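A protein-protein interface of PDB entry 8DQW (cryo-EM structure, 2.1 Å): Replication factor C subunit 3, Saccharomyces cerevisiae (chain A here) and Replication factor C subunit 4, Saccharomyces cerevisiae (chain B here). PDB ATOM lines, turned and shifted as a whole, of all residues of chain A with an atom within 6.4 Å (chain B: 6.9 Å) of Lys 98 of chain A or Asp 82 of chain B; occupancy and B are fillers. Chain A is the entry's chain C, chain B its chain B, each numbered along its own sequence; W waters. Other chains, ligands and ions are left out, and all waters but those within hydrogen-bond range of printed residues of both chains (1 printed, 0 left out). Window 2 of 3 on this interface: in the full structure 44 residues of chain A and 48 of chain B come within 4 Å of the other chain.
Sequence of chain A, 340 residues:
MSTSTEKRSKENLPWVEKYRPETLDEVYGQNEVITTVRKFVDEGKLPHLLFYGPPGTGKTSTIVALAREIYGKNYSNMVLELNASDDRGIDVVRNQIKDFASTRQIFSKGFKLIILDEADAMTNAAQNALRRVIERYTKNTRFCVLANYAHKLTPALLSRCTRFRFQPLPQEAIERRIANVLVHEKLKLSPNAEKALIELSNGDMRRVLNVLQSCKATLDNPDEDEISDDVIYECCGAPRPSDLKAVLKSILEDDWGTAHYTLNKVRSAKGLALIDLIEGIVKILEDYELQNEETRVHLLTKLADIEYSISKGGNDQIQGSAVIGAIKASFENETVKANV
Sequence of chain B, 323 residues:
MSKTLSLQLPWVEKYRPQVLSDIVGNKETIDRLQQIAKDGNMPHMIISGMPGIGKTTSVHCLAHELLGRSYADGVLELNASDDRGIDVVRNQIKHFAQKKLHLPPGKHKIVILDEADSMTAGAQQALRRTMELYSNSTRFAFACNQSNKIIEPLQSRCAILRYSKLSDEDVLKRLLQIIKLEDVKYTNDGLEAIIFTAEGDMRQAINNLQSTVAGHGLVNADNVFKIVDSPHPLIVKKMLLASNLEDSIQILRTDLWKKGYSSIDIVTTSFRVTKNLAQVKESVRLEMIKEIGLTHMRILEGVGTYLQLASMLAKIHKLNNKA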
ATOM      1  N   VAL A  92     -29.255  25.629  26.953  1.00  0.00           N
ATOM      2  CA  VAL A  92     -28.703  26.727  27.742  1.00  0.00           C
ATOM      3  C   VAL A  92     -27.325  26.351  28.273  1.00  0.00           C
ATOM      4  O   VAL A  92     -26.374  27.134  28.184  1.00  0.00           O
ATOM      5  CB  VAL A  92     -29.667  27.107  28.881  1.00  0.00           C
ATOM      6  CG1 VAL A  92     -28.950  27.935  29.941  1.00  0.00           C
ATOM      7  CG2 VAL A  92     -30.868  27.861  28.326  1.00  0.00           C
ATOM      8  N   VAL A  93     -27.192  25.135  28.805  1.00  0.00           N
ATOM      9  CA  VAL A  93     -25.894  24.684  29.303  1.00  0.00           C
ATOM     10  C   VAL A  93     -24.871  24.676  28.177  1.00  0.00           C
ATOM     11  O   VAL A  93     -23.727  25.115  28.352  1.00  0.00           O
ATOM     12  CB  VAL A  93     -26.024  23.293  29.953  1.00  0.00           C
ATOM     13  CG1 VAL A  93     -24.648  22.731  30.288  1.00  0.00           C
ATOM     14  CG2 VAL A  93     -26.893  23.364  31.195  1.00  0.00           C
ATOM     15  N   ARG A  94     -25.265  24.181  27.002  1.00  0.00           N
ATOM     16  CA  ARG A  94     -24.324  24.046  25.899  1.00  0.00           C
ATOM     17  C   ARG A  94     -23.871  25.406  25.377  1.00  0.00           C
ATOM     18  O   ARG A  94     -22.709  25.565  24.985  1.00  0.00           O
ATOM     19  CB  ARG A  94     -24.953  23.224  24.771  1.00  0.00           C
ATOM     20  CG  ARG A  94     -24.746  21.719  24.915  1.00  0.00           C
ATOM     21  CD  ARG A  94     -25.057  20.967  23.624  1.00  0.00           C
ATOM     22  NE  ARG A  94     -26.321  21.377  23.015  1.00  0.00           N
ATOM     23  CZ  ARG A  94     -27.426  20.640  22.979  1.00  0.00           C
ATOM     24  NH1 ARG A  94     -27.479  19.433  23.520  1.00  0.00           N
ATOM     25  NH2 ARG A  94     -28.510  21.128  22.380  1.00  0.00           N
ATOM     26  N   ASN A  95     -24.772  26.390  25.336  1.00  0.00           N
ATOM     27  CA  ASN A  95     -24.415  27.685  24.767  1.00  0.00           C
ATOM     28  C   ASN A  95     -23.992  28.711  25.816  1.00  0.00           C
ATOM     29  O   ASN A  95     -22.822  29.095  25.867  1.00  0.00           O
ATOM     30  CB  ASN A  95     -25.588  28.238  23.954  1.00  0.00           C
ATOM     31  CG  ASN A  95     -26.086  27.258  22.911  1.00  0.00           C
ATOM     32  OD1 ASN A  95     -27.216  26.774  22.984  1.00  0.00           O
ATOM     33  ND2 ASN A  95     -25.242  26.956  21.935  1.00  0.00           N
ATOM     34  N   GLN A  96     -24.909  29.110  26.699  1.00  0.00           N
ATOM     35  CA  GLN A  96     -24.670  30.290  27.526  1.00  0.00           C
ATOM     36  C   GLN A  96     -23.658  30.000  28.628  1.00  0.00           C
ATOM     37  O   GLN A  96     -22.657  30.716  28.773  1.00  0.00           O
ATOM     38  CB  GLN A  96     -25.991  30.780  28.122  1.00  0.00           C
ATOM     39  CG  GLN A  96     -25.839  31.782  29.257  1.00  0.00           C
ATOM     40  CD  GLN A  96     -27.161  32.398  29.671  1.00  0.00           C
ATOM     41  OE1 GLN A  96     -28.227  31.949  29.248  1.00  0.00           O
ATOM     42  NE2 GLN A  96     -27.099  33.429  30.505  1.00  0.00           N
ATOM     43  N   ILE A  97     -23.907  28.957  29.422  1.00  0.00           N
ATOM     44  CA  ILE A  97     -22.987  28.601  30.496  1.00  0.00           C
ATOM     45  C   ILE A  97     -21.627  28.236  29.920  1.00  0.00           C
ATOM     46  O   ILE A  97     -20.583  28.633  30.451  1.00  0.00           O
ATOM     47  CB  ILE A  97     -23.574  27.454  31.342  1.00  0.00           C
ATOM     48  CG1 ILE A  97     -24.806  27.942  32.110  1.00  0.00           C
ATOM     49  CG2 ILE A  97     -22.521  26.905  32.297  1.00  0.00           C
ATOM     50  CD1 ILE A  97     -25.670  26.832  32.678  1.00  0.00           C
ATOM     51  N   LYS A  98     -21.620  27.478  28.823  1.00  0.00           N
ATOM     52  CA  LYS A  98     -20.365  27.084  28.191  1.00  0.00           C
ATOM     53  C   LYS A  98     -19.559  28.302  27.754  1.00  0.00           C
ATOM     54  O   LYS A  98     -18.355  28.390  28.021  1.00  0.00           O
ATOM     55  CB  LYS A  98     -20.661  26.177  26.996  1.00  0.00           C
ATOM     56  CG  LYS A  98     -19.439  25.648  26.272  1.00  0.00           C
ATOM     57  CD  LYS A  98     -19.594  24.172  25.936  1.00  0.00           C
ATOM     58  CE  LYS A  98     -18.375  23.642  25.207  1.00  0.00           C
ATOM     59  NZ  LYS A  98     -18.435  22.166  24.995  1.00  0.00           N
ATOM     60  N   ASP A  99     -20.206  29.260  27.081  1.00  0.00           N
ATOM     61  CA  ASP A  99     -19.487  30.438  26.610  1.00  0.00           C
ATOM     62  C   ASP A  99     -19.000  31.296  27.770  1.00  0.00           C
ATOM     63  O   ASP A  99     -17.882  31.825  27.726  1.00  0.00           O
ATOM     64  CB  ASP A  99     -20.368  31.259  25.669  1.00  0.00           C
ATOM     65  CG  ASP A  99     -20.801  30.477  24.441  1.00  0.00           C
ATOM     66  OD1 ASP A  99     -21.976  30.602  24.035  1.00  0.00           O
ATOM     67  OD2 ASP A  99     -19.965  29.736  23.881  1.00  0.00           O
ATOM     68  N   PHE A 100     -19.815  31.455  28.815  1.00  0.00           N
ATOM     69  CA  PHE A 100     -19.366  32.236  29.963  1.00  0.00           C
ATOM     70  C   PHE A 100     -18.168  31.582  30.638  1.00  0.00           C
ATOM     71  O   PHE A 100     -17.199  32.262  30.997  1.00  0.00           O
ATOM     72  CB  PHE A 100     -20.500  32.416  30.971  1.00  0.00           C
ATOM     73  CG  PHE A 100     -20.114  33.245  32.166  1.00  0.00           C
ATOM     74  CD1 PHE A 100     -20.029  34.624  32.070  1.00  0.00           C
ATOM     75  CD2 PHE A 100     -19.813  32.643  33.376  1.00  0.00           C
ATOM     76  CE1 PHE A 100     -19.667  35.390  33.165  1.00  0.00           C
ATOM     77  CE2 PHE A 100     -19.451  33.403  34.474  1.00  0.00           C
ATOM     78  CZ  PHE A 100     -19.377  34.779  34.366  1.00  0.00           C
ATOM     79  N   ALA A 101     -18.211  30.260  30.816  1.00  0.00           N
ATOM     80  CA  ALA A 101     -17.135  29.565  31.510  1.00  0.00           C
ATOM     81  C   ALA A 101     -15.869  29.459  30.671  1.00  0.00           C
ATOM     82  O   ALA A 101     -14.792  29.226  31.230  1.00  0.00           O
ATOM     83  CB  ALA A 101     -17.592  28.165  31.921  1.00  0.00           C
ATOM     84  N   SER A 102     -15.971  29.624  29.353  1.00  0.00           N
ATOM     85  CA  SER A 102     -14.844  29.446  28.450  1.00  0.00           C
ATOM     86  C   SER A 102     -14.249  30.766  27.971  1.00  0.00           C
ATOM     87  O   SER A 102     -13.442  30.762  27.036  1.00  0.00           O
ATOM     88  CB  SER A 102     -15.268  28.603  27.246  1.00  0.00           C
ATOM     89  OG  SER A 102     -16.219  29.289  26.452  1.00  0.00           O
ATOM     90  N   THR A 103     -14.611  31.885  28.593  1.00  0.00           N
ATOM     91  CA  THR A 103     -14.116  33.199  28.208  1.00  0.00           C
ATOM     92  C   THR A 103     -13.340  33.827  29.360  1.00  0.00           C
ATOM     93  O   THR A 103     -13.526  33.476  30.528  1.00  0.00           O
ATOM     94  CB  THR A 103     -15.265  34.128  27.783  1.00  0.00           C
ATOM     95  OG1 THR A 103     -16.358  33.999  28.701  1.00  0.00           O
ATOM     96  CG2 THR A 103     -15.736  33.788  26.376  1.00  0.00           C
ATOM     97  N   ILE A 114     -19.962  30.856  38.627  1.00  0.00           N
ATOM     98  CA  ILE A 114     -21.281  30.527  38.103  1.00  0.00           C
ATOM     99  C   ILE A 114     -22.106  29.966  39.250  1.00  0.00           C
ATOM    100  O   ILE A 114     -21.746  28.938  39.838  1.00  0.00           O
ATOM    101  CB  ILE A 114     -21.206  29.525  36.940  1.00  0.00           C
ATOM    102  CG1 ILE A 114     -20.534  30.171  35.727  1.00  0.00           C
ATOM    103  CG2 ILE A 114     -22.601  29.026  36.577  1.00  0.00           C
ATOM    104  CD1 ILE A 114     -20.090  29.185  34.674  1.00  0.00           C
ATOM    105  N   ALA A 129     -24.804  17.279  30.969  1.00  0.00           N
ATOM    106  CA  ALA A 129     -23.968  18.147  30.145  1.00  0.00           C
ATOM    107  C   ALA A 129     -23.053  19.017  30.999  1.00  0.00           C
ATOM    108  O   ALA A 129     -21.973  19.410  30.547  1.00  0.00           O
ATOM    109  CB  ALA A 129     -24.843  19.019  29.246  1.00  0.00           C
ATOM    110  N   VAL A 133     -18.251  20.529  31.444  1.00  0.00           N
ATOM    111  CA  VAL A 133     -18.070  21.974  31.549  1.00  0.00           C
ATOM    112  C   VAL A 133     -17.411  22.317  32.877  1.00  0.00           C
ATOM    113  O   VAL A 133     -16.474  23.121  32.940  1.00  0.00           O
ATOM    114  CB  VAL A 133     -19.417  22.702  31.386  1.00  0.00           C
ATOM    115  CG1 VAL A 133     -19.223  24.209  31.519  1.00  0.00           C
ATOM    116  CG2 VAL A 133     -20.050  22.358  30.048  1.00  0.00           C
ATOM    117  N   ARG A 136     -13.539  20.713  32.744  1.00  0.00           N
ATOM    118  CA  ARG A 136     -12.519  21.228  31.834  1.00  0.00           C
ATOM    119  C   ARG A 136     -12.116  22.656  32.184  1.00  0.00           C
ATOM    120  O   ARG A 136     -10.936  23.013  32.088  1.00  0.00           O
ATOM    121  CB  ARG A 136     -13.019  21.152  30.392  1.00  0.00           C
ATOM    122  CG  ARG A 136     -12.308  22.106  29.440  1.00  0.00           C
ATOM    123  CD  ARG A 136     -12.484  21.691  27.991  1.00  0.00           C
ATOM    124  NE  ARG A 136     -13.645  22.329  27.383  1.00  0.00           N
ATOM    125  CZ  ARG A 136     -14.831  21.754  27.226  1.00  0.00           C
ATOM    126  NH1 ARG A 136     -15.064  20.516  27.633  1.00  0.00           N
ATOM    127  NH2 ARG A 136     -15.811  22.442  26.650  1.00  0.00           N
ATOM    128  N   TYR A 137     -13.077  23.491  32.583  1.00  0.00           N
ATOM    129  CA  TYR A 137     -12.832  24.908  32.831  1.00  0.00           C
ATOM    130  C   TYR A 137     -12.645  25.218  34.312  1.00  0.00           C
ATOM    131  O   TYR A 137     -12.927  26.339  34.751  1.00  0.00           O
ATOM    132  CB  TYR A 137     -13.979  25.738  32.254  1.00  0.00           C
ATOM    133  CG  TYR A 137     -14.151  25.567  30.763  1.00  0.00           C
ATOM    134  CD1 TYR A 137     -13.168  25.995  29.882  1.00  0.00           C
ATOM    135  CD2 TYR A 137     -15.286  24.965  30.237  1.00  0.00           C
ATOM    136  CE1 TYR A 137     -13.314  25.841  28.521  1.00  0.00           C
ATOM    137  CE2 TYR A 137     -15.441  24.802  28.873  1.00  0.00           C
ATOM    138  CZ  TYR A 137     -14.450  25.243  28.020  1.00  0.00           C
ATOM    139  OH  TYR A 137     -14.590  25.088  26.661  1.00  0.00           O
ATOM    140  N   GLU B  77     -12.232  13.882  20.848  1.00  0.00           N
ATOM    141  CA  GLU B  77     -12.934  13.755  22.119  1.00  0.00           C
ATOM    142  C   GLU B  77     -14.277  14.467  22.042  1.00  0.00           C
ATOM    143  O   GLU B  77     -14.352  15.610  21.582  1.00  0.00           O
ATOM    144  CB  GLU B  77     -12.101  14.331  23.265  1.00  0.00           C
ATOM    145  CG  GLU B  77     -12.417  13.726  24.623  1.00  0.00           C
ATOM    146  CD  GLU B  77     -13.730  14.225  25.194  1.00  0.00           C
ATOM    147  OE1 GLU B  77     -13.989  15.444  25.115  1.00  0.00           O
ATOM    148  OE2 GLU B  77     -14.503  13.399  25.723  1.00  0.00           O
ATOM    149  N   LEU B  78     -15.331  13.791  22.497  1.00  0.00           N
ATOM    150  CA  LEU B  78     -16.663  14.376  22.555  1.00  0.00           C
ATOM    151  C   LEU B  78     -17.378  13.875  23.801  1.00  0.00           C
ATOM    152  O   LEU B  78     -17.303  12.687  24.131  1.00  0.00           O
ATOM    153  CB  LEU B  78     -17.483  14.032  21.304  1.00  0.00           C
ATOM    154  CG  LEU B  78     -17.064  14.741  20.013  1.00  0.00           C
ATOM    155  CD1 LEU B  78     -17.819  14.166  18.824  1.00  0.00           C
ATOM    156  CD2 LEU B  78     -17.288  16.244  20.115  1.00  0.00           C
ATOM    157  N   ASN B  79     -18.074  14.783  24.484  1.00  0.00           N
ATOM    158  CA  ASN B  79     -18.799  14.457  25.703  1.00  0.00           C
ATOM    159  C   ASN B  79     -20.185  15.089  25.639  1.00  0.00           C
ATOM    160  O   ASN B  79     -20.565  15.706  24.640  1.00  0.00           O
ATOM    161  CB  ASN B  79     -18.030  14.923  26.945  1.00  0.00           C
ATOM    162  CG  ASN B  79     -17.603  16.375  26.856  1.00  0.00           C
ATOM    163  OD1 ASN B  79     -18.437  17.280  26.863  1.00  0.00           O
ATOM    164  ND2 ASN B  79     -16.298  16.603  26.777  1.00  0.00           N
ATOM    165  N   ALA B  80     -20.944  14.936  26.728  1.00  0.00           N
ATOM    166  CA  ALA B  80     -22.325  15.402  26.749  1.00  0.00           C
ATOM    167  C   ALA B  80     -22.433  16.918  26.640  1.00  0.00           C
ATOM    168  O   ALA B  80     -23.519  17.429  26.346  1.00  0.00           O
ATOM    169  CB  ALA B  80     -23.018  14.925  28.026  1.00  0.00           C
ATOM    170  N   SER B  81     -21.341  17.648  26.869  1.00  0.00           N
ATOM    171  CA  SER B  81     -21.365  19.101  26.769  1.00  0.00           C
ATOM    172  C   SER B  81     -21.222  19.603  25.338  1.00  0.00           C
ATOM    173  O   SER B  81     -21.392  20.802  25.101  1.00  0.00           O
ATOM    174  CB  SER B  81     -20.252  19.703  27.633  1.00  0.00           C
ATOM    175  OG  SER B  81     -19.046  19.826  26.902  1.00  0.00           O
ATOM    176  N   ASP B  82     -20.913  18.726  24.387  1.00  0.00           N
ATOM    177  CA  ASP B  82     -20.781  19.087  22.985  1.00  0.00           C
ATOM    178  C   ASP B  82     -21.991  18.598  22.201  1.00  0.00           C
ATOM    179  O   ASP B  82     -22.774  17.768  22.674  1.00  0.00           O
ATOM    180  CB  ASP B  82     -19.504  18.490  22.383  1.00  0.00           C
ATOM    181  CG  ASP B  82     -18.266  18.816  23.193  1.00  0.00           C
ATOM    182  OD1 ASP B  82     -17.985  20.016  23.395  1.00  0.00           O
ATOM    183  OD2 ASP B  82     -17.575  17.872  23.630  1.00  0.00           O
ATOM    184  N   ASP B  83     -22.140  19.128  20.990  1.00  0.00           N
ATOM    185  CA  ASP B  83     -23.150  18.614  20.076  1.00  0.00           C
ATOM    186  C   ASP B  83     -22.750  17.218  19.613  1.00  0.00           C
ATOM    187  O   ASP B  83     -21.644  17.017  19.104  1.00  0.00           O
ATOM    188  CB  ASP B  83     -23.311  19.546  18.875  1.00  0.00           C
ATOM    189  CG  ASP B  83     -24.458  19.137  17.967  1.00  0.00           C
ATOM    190  OD1 ASP B  83     -25.223  18.222  18.342  1.00  0.00           O
ATOM    191  OD2 ASP B  83     -24.595  19.730  16.877  1.00  0.00           O
ATOM    192  N   ARG B  84     -23.653  16.255  19.795  1.00  0.00           N
ATOM    193  CA  ARG B  84     -23.374  14.870  19.435  1.00  0.00           C
ATOM    194  C   ARG B  84     -24.564  14.227  18.734  1.00  0.00           C
ATOM    195  O   ARG B  84     -24.776  13.015  18.848  1.00  0.00           O
ATOM    196  CB  ARG B  84     -22.996  14.051  20.671  1.00  0.00           C
ATOM    197  CG  ARG B  84     -21.703  14.487  21.334  1.00  0.00           C
ATOM    198  CD  ARG B  84     -21.190  13.416  22.278  1.00  0.00           C
ATOM    199  NE  ARG B  84     -22.187  13.050  23.278  1.00  0.00           N
ATOM    200  CZ  ARG B  84     -21.917  12.414  24.409  1.00  0.00           C
ATOM    201  NH1 ARG B  84     -20.690  12.020  24.707  1.00  0.00           N
ATOM    202  NH2 ARG B  84     -22.906  12.159  25.261  1.00  0.00           N
ATOM    203  N   GLY B  85     -25.343  15.017  18.004  1.00  0.00           N
ATOM    204  CA  GLY B  85     -26.505  14.505  17.318  1.00  0.00           C
ATOM    205  C   GLY B  85     -26.124  13.697  16.090  1.00  0.00           C
ATOM    206  O   GLY B  85     -24.957  13.424  15.808  1.00  0.00           O
ATOM    207  N   VAL B  88     -23.742  15.285  13.666  1.00  0.00           N
ATOM    208  CA  VAL B  88     -22.346  15.219  14.085  1.00  0.00           C
ATOM    209  C   VAL B  88     -21.730  13.893  13.660  1.00  0.00           C
ATOM    210  O   VAL B  88     -20.624  13.858  13.111  1.00  0.00           O
ATOM    211  CB  VAL B  88     -22.230  15.445  15.604  1.00  0.00           C
ATOM    212  CG1 VAL B  88     -20.776  15.360  16.050  1.00  0.00           C
ATOM    213  CG2 VAL B  88     -22.828  16.795  15.979  1.00  0.00           C
HETATM  214  O   HOH W   1     -25.102  17.551  23.868  1.00  0.00           O
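OG of Ser 81 of chain B is in hydrogen-bond range of OD1 of Asn 79 of chain B, at 2.6 Å. The side-chain carboxylate (OD2) of Asp 82 of chain B sits at hydrogen-bond distance from the backbone NH (N) of Asn 79 of chain B (3.2 Å). O of Val 93 of chain A sits at hydrogen-bond distance from N of Lys 98 of chain A (3.2 Å). The backbone carbonyl oxygen (O) of Lys 98 of chain A is in hydrogen-bond range of the side-chain hydroxyl (OG) of Ser 102 of chain A (2.8 Å).
Of the 10 printed residues of chain B, 3 touch a printed residue of chain A. Hydrophobic or aromatic side chains of chain A that line the printed part of chain B: Ala 129 and Val 133. Among the printed residues, 6 pairs touch across the chains. Among the printed residues, Asp or Glu carboxylates within 4 Å of a Lys or Arg side-chain nitrogen of the other chain: Lys 98 of chain A with Asp 82 of chain B.
Printed residues of chain B within 4 Å of Arg 94 of chain A: Ser 81 (3.5 Å). Printed residues of chain B within 4 Å of Val 133 of chain A: Ser 81 (3.6 Å). Leu 78 of chain B touches none of the printed residues of chain A. Of the printed residues of chain A, Ser 81 of chain B touches Arg 94 (3.5 Å), Lys 98 (3.1 Å), Ala 129 (3.4 Å) and Val 133 (3.6 Å). Asp 82 of chain B touches one residue of chain A. Gly 85 of chain B touches none of the printed residues of chain A. The nearest residue of chain A that does not touch Asp 82 of chain B is Arg 94 of chain A (4.04 Å).
Among the printed residues, pairs that only touch across the chains: Ala 129 of chain A with Ser 81 of chain B, Arg 94 of chain A with Ser 81 of chain B, Ala 129 of chain A with Ala 80 of chain B and Val 133 of chain A with Ser 81 of chain B.
OG of Ser 81 of chain B is in hydrogen-bond range of NZ of Lys 98 of chain A, 3.1 Å away. NZ of Lys 98 of chain A is in salt-bridge range of OD1 of Asp 82 of chain B (2.7 Å).
Water W1 lies within hydrogen-bond range of O of Asp 82 of chain B (2.6 Å), O of Ala 80 of chain B (2.9 Å) and NH1 of Arg 94 of chain A (3.1 Å).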
